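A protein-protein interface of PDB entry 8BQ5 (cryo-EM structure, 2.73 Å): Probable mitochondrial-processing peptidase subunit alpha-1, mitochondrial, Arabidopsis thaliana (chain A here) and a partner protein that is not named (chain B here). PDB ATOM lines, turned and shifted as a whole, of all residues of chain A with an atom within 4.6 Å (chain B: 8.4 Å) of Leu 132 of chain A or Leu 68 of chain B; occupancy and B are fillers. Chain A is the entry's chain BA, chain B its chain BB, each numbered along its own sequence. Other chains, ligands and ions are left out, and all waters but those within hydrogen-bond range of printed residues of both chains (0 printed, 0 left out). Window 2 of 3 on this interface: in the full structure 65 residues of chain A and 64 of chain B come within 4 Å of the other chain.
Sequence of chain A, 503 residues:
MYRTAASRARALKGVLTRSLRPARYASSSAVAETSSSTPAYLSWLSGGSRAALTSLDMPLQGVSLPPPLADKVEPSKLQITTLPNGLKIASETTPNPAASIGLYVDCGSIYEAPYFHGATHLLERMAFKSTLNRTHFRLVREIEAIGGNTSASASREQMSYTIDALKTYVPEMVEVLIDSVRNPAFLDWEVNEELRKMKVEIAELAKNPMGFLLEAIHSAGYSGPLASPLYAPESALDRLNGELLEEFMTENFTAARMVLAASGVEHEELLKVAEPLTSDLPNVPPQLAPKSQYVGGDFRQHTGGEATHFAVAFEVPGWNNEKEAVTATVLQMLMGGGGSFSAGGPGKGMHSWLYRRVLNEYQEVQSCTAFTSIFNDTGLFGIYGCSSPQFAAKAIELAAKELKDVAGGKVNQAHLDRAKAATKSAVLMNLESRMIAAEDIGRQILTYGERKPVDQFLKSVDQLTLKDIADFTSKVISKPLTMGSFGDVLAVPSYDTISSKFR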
ATOM      1  N   THR A 131       5.885  10.567  17.082  1.00  0.00           N
ATOM      2  CA  THR A 131       5.911   9.835  15.827  1.00  0.00           C
ATOM      3  C   THR A 131       4.632  10.122  15.047  1.00  0.00           C
ATOM      4  O   THR A 131       3.766  10.887  15.482  1.00  0.00           O
ATOM      5  CB  THR A 131       6.075   8.335  16.079  1.00  0.00           C
ATOM      6  OG1 THR A 131       4.985   7.859  16.874  1.00  0.00           O
ATOM      7  CG2 THR A 131       7.380   8.059  16.809  1.00  0.00           C
ATOM      8  N   LEU A 132       4.518   9.500  13.874  1.00  0.00           N
ATOM      9  CA  LEU A 132       3.302   9.639  13.085  1.00  0.00           C
ATOM     10  C   LEU A 132       2.127   8.879  13.679  1.00  0.00           C
ATOM     11  O   LEU A 132       0.987   9.122  13.271  1.00  0.00           O
ATOM     12  CB  LEU A 132       3.546   9.167  11.652  1.00  0.00           C
ATOM     13  CG  LEU A 132       4.732   9.786  10.913  1.00  0.00           C
ATOM     14  CD1 LEU A 132       4.930   9.097   9.577  1.00  0.00           C
ATOM     15  CD2 LEU A 132       4.515  11.275  10.722  1.00  0.00           C
ATOM     16  N   ASN A 133       2.372   7.976  14.629  1.00  0.00           N
ATOM     17  CA  ASN A 133       1.325   7.134  15.184  1.00  0.00           C
ATOM     18  C   ASN A 133       1.026   7.417  16.649  1.00  0.00           C
ATOM     19  O   ASN A 133      -0.052   7.042  17.124  1.00  0.00           O
ATOM     20  CB  ASN A 133       1.702   5.656  15.019  1.00  0.00           C
ATOM     21  CG  ASN A 133       1.946   5.280  13.571  1.00  0.00           C
ATOM     22  OD1 ASN A 133       1.094   5.493  12.711  1.00  0.00           O
ATOM     23  ND2 ASN A 133       3.122   4.731  13.293  1.00  0.00           N
ATOM     24  N   ARG A 134       1.938   8.058  17.374  1.00  0.00           N
ATOM     25  CA  ARG A 134       1.717   8.369  18.776  1.00  0.00           C
ATOM     26  C   ARG A 134       2.482   9.634  19.124  1.00  0.00           C
ATOM     27  O   ARG A 134       3.553   9.893  18.567  1.00  0.00           O
ATOM     28  CB  ARG A 134       2.160   7.218  19.684  1.00  0.00           C
ATOM     29  CG  ARG A 134       3.339   6.441  19.143  1.00  0.00           C
ATOM     30  CD  ARG A 134       3.910   5.492  20.172  1.00  0.00           C
ATOM     31  NE  ARG A 134       2.990   4.404  20.476  1.00  0.00           N
ATOM     32  CZ  ARG A 134       3.092   3.181  19.976  1.00  0.00           C
ATOM     33  NH1 ARG A 134       4.046   2.864  19.117  1.00  0.00           N
ATOM     34  NH2 ARG A 134       2.210   2.255  20.342  1.00  0.00           N
ATOM     35  N   ASN A 183       9.256   5.984  11.842  1.00  0.00           N
ATOM     36  CA  ASN A 183       8.274   7.031  11.563  1.00  0.00           C
ATOM     37  C   ASN A 183       8.400   8.200  12.534  1.00  0.00           C
ATOM     38  O   ASN A 183       7.485   8.460  13.321  1.00  0.00           O
ATOM     39  CB  ASN A 183       6.859   6.459  11.621  1.00  0.00           C
ATOM     40  CG  ASN A 183       6.745   5.112  10.951  1.00  0.00           C
ATOM     41  OD1 ASN A 183       6.248   4.154  11.540  1.00  0.00           O
ATOM     42  ND2 ASN A 183       7.197   5.031   9.705  1.00  0.00           N
ATOM     43  N   PRO A 184       9.506   8.940  12.497  1.00  0.00           N
ATOM     44  CA  PRO A 184       9.566  10.181  13.276  1.00  0.00           C
ATOM     45  C   PRO A 184       8.679  11.246  12.651  1.00  0.00           C
ATOM     46  O   PRO A 184       8.512  11.304  11.431  1.00  0.00           O
ATOM     47  CB  PRO A 184      11.047  10.578  13.218  1.00  0.00           C
ATOM     48  CG  PRO A 184      11.757   9.416  12.598  1.00  0.00           C
ATOM     49  CD  PRO A 184      10.753   8.717  11.752  1.00  0.00           C
ATOM     50  N   ALA A 185       8.105  12.093  13.503  1.00  0.00           N
ATOM     51  CA  ALA A 185       7.286  13.196  13.022  1.00  0.00           C
ATOM     52  C   ALA A 185       8.098  14.454  12.758  1.00  0.00           C
ATOM     53  O   ALA A 185       7.766  15.212  11.838  1.00  0.00           O
ATOM     54  CB  ALA A 185       6.169  13.503  14.023  1.00  0.00           C
ATOM     55  N   LEU A 187       8.358  17.278  14.362  1.00  0.00           N
ATOM     56  CA  LEU A 187       7.578  18.499  14.501  1.00  0.00           C
ATOM     57  C   LEU A 187       8.490  19.674  14.830  1.00  0.00           C
ATOM     58  O   LEU A 187       9.462  19.537  15.579  1.00  0.00           O
ATOM     59  CB  LEU A 187       6.516  18.334  15.587  1.00  0.00           C
ATOM     60  CG  LEU A 187       5.705  17.042  15.550  1.00  0.00           C
ATOM     61  CD1 LEU A 187       4.933  16.873  16.845  1.00  0.00           C
ATOM     62  CD2 LEU A 187       4.768  17.028  14.354  1.00  0.00           C
ATOM     63  N   ILE B  61       2.265  23.315   6.660  1.00  0.00           N
ATOM     64  CA  ILE B  61       1.981  22.903   8.030  1.00  0.00           C
ATOM     65  C   ILE B  61       0.620  22.222   8.118  1.00  0.00           C
ATOM     66  O   ILE B  61       0.429  21.310   8.931  1.00  0.00           O
ATOM     67  CB  ILE B  61       2.095  24.106   8.991  1.00  0.00           C
ATOM     68  CG1 ILE B  61       2.252  23.629  10.436  1.00  0.00           C
ATOM     69  CG2 ILE B  61       0.897  25.034   8.873  1.00  0.00           C
ATOM     70  CD1 ILE B  61       3.344  22.603  10.628  1.00  0.00           C
ATOM     71  N   LYS B  62      -0.341  22.636   7.288  1.00  0.00           N
ATOM     72  CA  LYS B  62      -1.655  22.004   7.308  1.00  0.00           C
ATOM     73  C   LYS B  62      -1.587  20.575   6.785  1.00  0.00           C
ATOM     74  O   LYS B  62      -2.261  19.683   7.312  1.00  0.00           O
ATOM     75  CB  LYS B  62      -2.646  22.831   6.491  1.00  0.00           C
ATOM     76  CG  LYS B  62      -3.291  23.964   7.269  1.00  0.00           C
ATOM     77  CD  LYS B  62      -4.455  24.566   6.503  1.00  0.00           C
ATOM     78  CE  LYS B  62      -3.970  25.384   5.319  1.00  0.00           C
ATOM     79  NZ  LYS B  62      -5.083  26.143   4.687  1.00  0.00           N
ATOM     80  N   ASN B  63      -0.786  20.340   5.744  1.00  0.00           N
ATOM     81  CA  ASN B  63      -0.628  18.988   5.221  1.00  0.00           C
ATOM     82  C   ASN B  63       0.094  18.091   6.220  1.00  0.00           C
ATOM     83  O   ASN B  63      -0.223  16.902   6.340  1.00  0.00           O
ATOM     84  CB  ASN B  63       0.121  19.024   3.890  1.00  0.00           C
ATOM     85  CG  ASN B  63      -0.769  19.433   2.735  1.00  0.00           C
ATOM     86  OD1 ASN B  63      -1.626  20.305   2.875  1.00  0.00           O
ATOM     87  ND2 ASN B  63      -0.570  18.803   1.585  1.00  0.00           N
ATOM     88  N   LYS B  64       1.077  18.641   6.934  1.00  0.00           N
ATOM     89  CA  LYS B  64       1.778  17.868   7.954  1.00  0.00           C
ATOM     90  C   LYS B  64       0.835  17.449   9.075  1.00  0.00           C
ATOM     91  O   LYS B  64       0.875  16.302   9.535  1.00  0.00           O
ATOM     92  CB  LYS B  64       2.944  18.679   8.513  1.00  0.00           C
ATOM     93  CG  LYS B  64       4.275  17.963   8.458  1.00  0.00           C
ATOM     94  CD  LYS B  64       4.337  16.846   9.481  1.00  0.00           C
ATOM     95  CE  LYS B  64       5.741  16.280   9.584  1.00  0.00           C
ATOM     96  NZ  LYS B  64       5.737  14.898  10.135  1.00  0.00           N
ATOM     97  N   ILE B  65      -0.022  18.368   9.523  1.00  0.00           N
ATOM     98  CA  ILE B  65      -0.947  18.067  10.612  1.00  0.00           C
ATOM     99  C   ILE B  65      -1.950  17.004  10.182  1.00  0.00           C
ATOM    100  O   ILE B  65      -2.354  16.150  10.981  1.00  0.00           O
ATOM    101  CB  ILE B  65      -1.646  19.358  11.080  1.00  0.00           C
ATOM    102  CG1 ILE B  65      -0.690  20.209  11.914  1.00  0.00           C
ATOM    103  CG2 ILE B  65      -2.901  19.046  11.881  1.00  0.00           C
ATOM    104  CD1 ILE B  65      -1.155  21.630  12.085  1.00  0.00           C
ATOM    105  N   LYS B  66      -2.361  17.033   8.911  1.00  0.00           N
ATOM    106  CA  LYS B  66      -3.352  16.074   8.431  1.00  0.00           C
ATOM    107  C   LYS B  66      -2.834  14.644   8.517  1.00  0.00           C
ATOM    108  O   LYS B  66      -3.573  13.733   8.908  1.00  0.00           O
ATOM    109  CB  LYS B  66      -3.753  16.406   6.995  1.00  0.00           C
ATOM    110  CG  LYS B  66      -5.197  16.849   6.844  1.00  0.00           C
ATOM    111  CD  LYS B  66      -5.442  17.474   5.481  1.00  0.00           C
ATOM    112  CE  LYS B  66      -4.596  18.719   5.281  1.00  0.00           C
ATOM    113  NZ  LYS B  66      -4.879  19.376   3.976  1.00  0.00           N
ATOM    114  N   LYS B  67      -1.571  14.425   8.162  1.00  0.00           N
ATOM    115  CA  LYS B  67      -1.003  13.084   8.157  1.00  0.00           C
ATOM    116  C   LYS B  67      -0.790  12.525   9.559  1.00  0.00           C
ATOM    117  O   LYS B  67      -0.499  11.331   9.696  1.00  0.00           O
ATOM    118  CB  LYS B  67       0.313  13.076   7.370  1.00  0.00           C
ATOM    119  CG  LYS B  67       1.561  13.308   8.200  1.00  0.00           C
ATOM    120  CD  LYS B  67       2.768  13.536   7.301  1.00  0.00           C
ATOM    121  CE  LYS B  67       3.324  12.225   6.766  1.00  0.00           C
ATOM    122  NZ  LYS B  67       4.802  12.279   6.589  1.00  0.00           N
ATOM    123  N   LEU B  68      -0.931  13.347  10.596  1.00  0.00           N
ATOM    124  CA  LEU B  68      -0.918  12.877  11.973  1.00  0.00           C
ATOM    125  C   LEU B  68      -2.293  12.420  12.441  1.00  0.00           C
ATOM    126  O   LEU B  68      -2.407  11.852  13.530  1.00  0.00           O
ATOM    127  CB  LEU B  68      -0.402  13.976  12.906  1.00  0.00           C
ATOM    128  CG  LEU B  68       1.065  14.392  12.795  1.00  0.00           C
ATOM    129  CD1 LEU B  68       1.274  15.725  13.493  1.00  0.00           C
ATOM    130  CD2 LEU B  68       1.985  13.329  13.373  1.00  0.00           C
ATOM    131  N   GLU B  69      -3.335  12.660  11.646  1.00  0.00           N
ATOM    132  CA  GLU B  69      -4.699  12.303  12.005  1.00  0.00           C
ATOM    133  C   GLU B  69      -5.068  10.877  11.619  1.00  0.00           C
ATOM    134  O   GLU B  69      -6.145  10.409  12.006  1.00  0.00           O
ATOM    135  CB  GLU B  69      -5.685  13.271  11.344  1.00  0.00           C
ATOM    136  CG  GLU B  69      -5.842  14.600  12.059  1.00  0.00           C
ATOM    137  CD  GLU B  69      -7.161  14.713  12.792  1.00  0.00           C
ATOM    138  OE1 GLU B  69      -7.562  13.734  13.455  1.00  0.00           O
ATOM    139  OE2 GLU B  69      -7.805  15.780  12.697  1.00  0.00           O
ATOM    140  N   ASN B  70      -4.217  10.181  10.869  1.00  0.00           N
ATOM    141  CA  ASN B  70      -4.491   8.822  10.401  1.00  0.00           C
ATOM    142  C   ASN B  70      -3.306   7.928  10.741  1.00  0.00           C
ATOM    143  O   ASN B  70      -2.477   7.617   9.875  1.00  0.00           O
ATOM    144  CB  ASN B  70      -4.785   8.804   8.900  1.00  0.00           C
ATOM    145  CG  ASN B  70      -5.647   9.972   8.463  1.00  0.00           C
ATOM    146  OD1 ASN B  70      -5.261  10.753   7.594  1.00  0.00           O
ATOM    147  ND2 ASN B  70      -6.826  10.093   9.062  1.00  0.00           N
ATOM    148  N   PRO B  71      -3.193   7.499  11.995  1.00  0.00           N
ATOM    149  CA  PRO B  71      -2.085   6.615  12.374  1.00  0.00           C
ATOM    150  C   PRO B  71      -2.251   5.219  11.798  1.00  0.00           C
ATOM    151  O   PRO B  71      -3.358   4.771  11.486  1.00  0.00           O
ATOM    152  CB  PRO B  71      -2.158   6.593  13.905  1.00  0.00           C
ATOM    153  CG  PRO B  71      -3.581   6.894  14.211  1.00  0.00           C
ATOM    154  CD  PRO B  71      -4.042   7.846  13.147  1.00  0.00           C
ATOM    155  N   ASP B  72      -1.123   4.525  11.663  1.00  0.00           N
ATOM    156  CA  ASP B  72      -1.116   3.149  11.182  1.00  0.00           C
ATOM    157  C   ASP B  72      -1.262   2.199  12.364  1.00  0.00           C
ATOM    158  O   ASP B  72      -0.411   2.176  13.258  1.00  0.00           O
ATOM    159  CB  ASP B  72       0.173   2.864  10.415  1.00  0.00           C
ATOM    160  CG  ASP B  72       0.138   1.534   9.690  1.00  0.00           C
ATOM    161  OD1 ASP B  72       1.213   1.058   9.268  1.00  0.00           O
ATOM    162  OD2 ASP B  72      -0.963   0.965   9.538  1.00  0.00           O
ATOM    163  N   PHE B  75       1.401  -0.262  14.356  1.00  0.00           N
ATOM    164  CA  PHE B  75       2.278   0.102  15.458  1.00  0.00           C
ATOM    165  C   PHE B  75       1.523   0.490  16.723  1.00  0.00           C
ATOM    166  O   PHE B  75       2.103   1.133  17.601  1.00  0.00           O
ATOM    167  CB  PHE B  75       3.192   1.257  15.040  1.00  0.00           C
ATOM    168  CG  PHE B  75       4.069   0.949  13.862  1.00  0.00           C
ATOM    169  CD1 PHE B  75       3.622   1.168  12.569  1.00  0.00           C
ATOM    170  CD2 PHE B  75       5.350   0.458  14.046  1.00  0.00           C
ATOM    171  CE1 PHE B  75       4.430   0.891  11.486  1.00  0.00           C
ATOM    172  CE2 PHE B  75       6.164   0.181  12.966  1.00  0.00           C
ATOM    173  CZ  PHE B  75       5.702   0.398  11.684  1.00  0.00           C
ATOM    174  N   LEU B  76       0.250   0.124  16.839  1.00  0.00           N
ATOM    175  CA  LEU B  76      -0.576   0.565  17.960  1.00  0.00           C
ATOM    176  C   LEU B  76      -1.397  -0.598  18.506  1.00  0.00           C
ATOM    177  O   LEU B  76      -2.590  -0.471  18.781  1.00  0.00           O
ATOM    178  CB  LEU B  76      -1.481   1.720  17.541  1.00  0.00           C
ATOM    179  CG  LEU B  76      -0.837   3.104  17.427  1.00  0.00           C
ATOM    180  CD1 LEU B  76      -1.675   4.010  16.543  1.00  0.00           C
ATOM    181  CD2 LEU B  76      -0.637   3.724  18.797  1.00  0.00           C
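Among the printed residues, merely in contact across the chains: Thr 131 of chain A with Leu 68 of chain B (3.7 Å), Leu 132 of chain A with Lys 64 of chain B (3.9 Å), Leu 132 of chain A with Leu 68 of chain B (3.9 Å), Asn 133 of chain A with Pro 71 of chain B (3.4 Å), Asn 133 of chain A with Phe 75 of chain B (3.7 Å), Asn 133 of chain A with Leu 76 of chain B (3.5 Å), Arg 134 of chain A with Leu 76 of chain B (3.6 Å), Asn 183 of chain A with Phe 75 of chain B (3.7 Å) and Leu 187 of chain A with Leu 68 of chain B (3.8 Å).
Of the 14 printed residues of chain B, 6 touch a printed residue of chain A.
Hydrophobic or aromatic side chains of chain B within 4 Å of the printed part of chain A: Leu 68, Pro 71, Phe 75 and Leu 76.
Of the 8 printed residues of chain A, 7 touch a printed residue of chain B.
Hydrophobic or aromatic side chains of chain A that line the printed part of chain B: Leu 132 and Leu 187.
Along chain A the printed residues that touch a printed residue of chain B span positions 131 to 187.
Among the printed residues, 12 pairs touch across the chains.
Among the printed residues, no Asp or Glu carboxylate lies within 4 Å of a Lys or Arg side-chain nitrogen of the other chain.
The side-chain amide oxygen (OD1) of Asn 133 of chain A is in hydrogen-bond range of the backbone NH (N) of Asp 72 of chain B (2.6 Å).
NH2 of Arg 134 of chain A lies within hydrogen-bond range of O of Phe 75 of chain B (3.0 Å).
The backbone carbonyl oxygen (O) of Ala 185 of chain A lies within hydrogen-bond range of the side-chain amino group (NZ) of Lys 64 of chain B (2.7 Å).
The backbone carbonyl oxygen of Asn 183 of chain A sits at hydrogen-bond distance from the backbone NH of Leu 132 of chain A, at 3.2 Å.
OG1 of Thr 131 of chain A is in hydrogen-bond range of O of Arg 134 of chain A.
OG1 of Thr 131 of chain A sits close to N of Asn 133 of chain A (3.4 Å).
Of the printed residues of chain B, Thr 131 of chain A touches Leu 68.
Of the printed residues of chain B, Asn 133 of chain A touches Pro 71 (3.4 Å), Asp 72 (2.6 Å), Phe 75 (3.7 Å) and Leu 76 (3.5 Å).
Of the printed residues of chain B, Asn 183 of chain A touches Phe 75.
Of the printed residues of chain B, Ala 185 of chain A touches Lys 64.
Lys 66 of chain B touches none of the printed residues of chain A.
Of chain A, only Thr 131, Leu 132 and Leu 187 come within 4 Å of Leu 68 of chain B.
Of the printed residues of chain A, Asp 72 of chain B touches Asn 133.
The nearest residue of chain B that does not touch Leu 132 of chain A is Pro 71 of chain B (4.1 Å).
The nearest residue of chain A that does not touch Leu 68 of chain B is Ala 185 of chain A (4.2 Å).
The nearest printed residue of chain A that does not touch Lys 64 of chain B is Pro 184 of chain A (4.7 Å).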
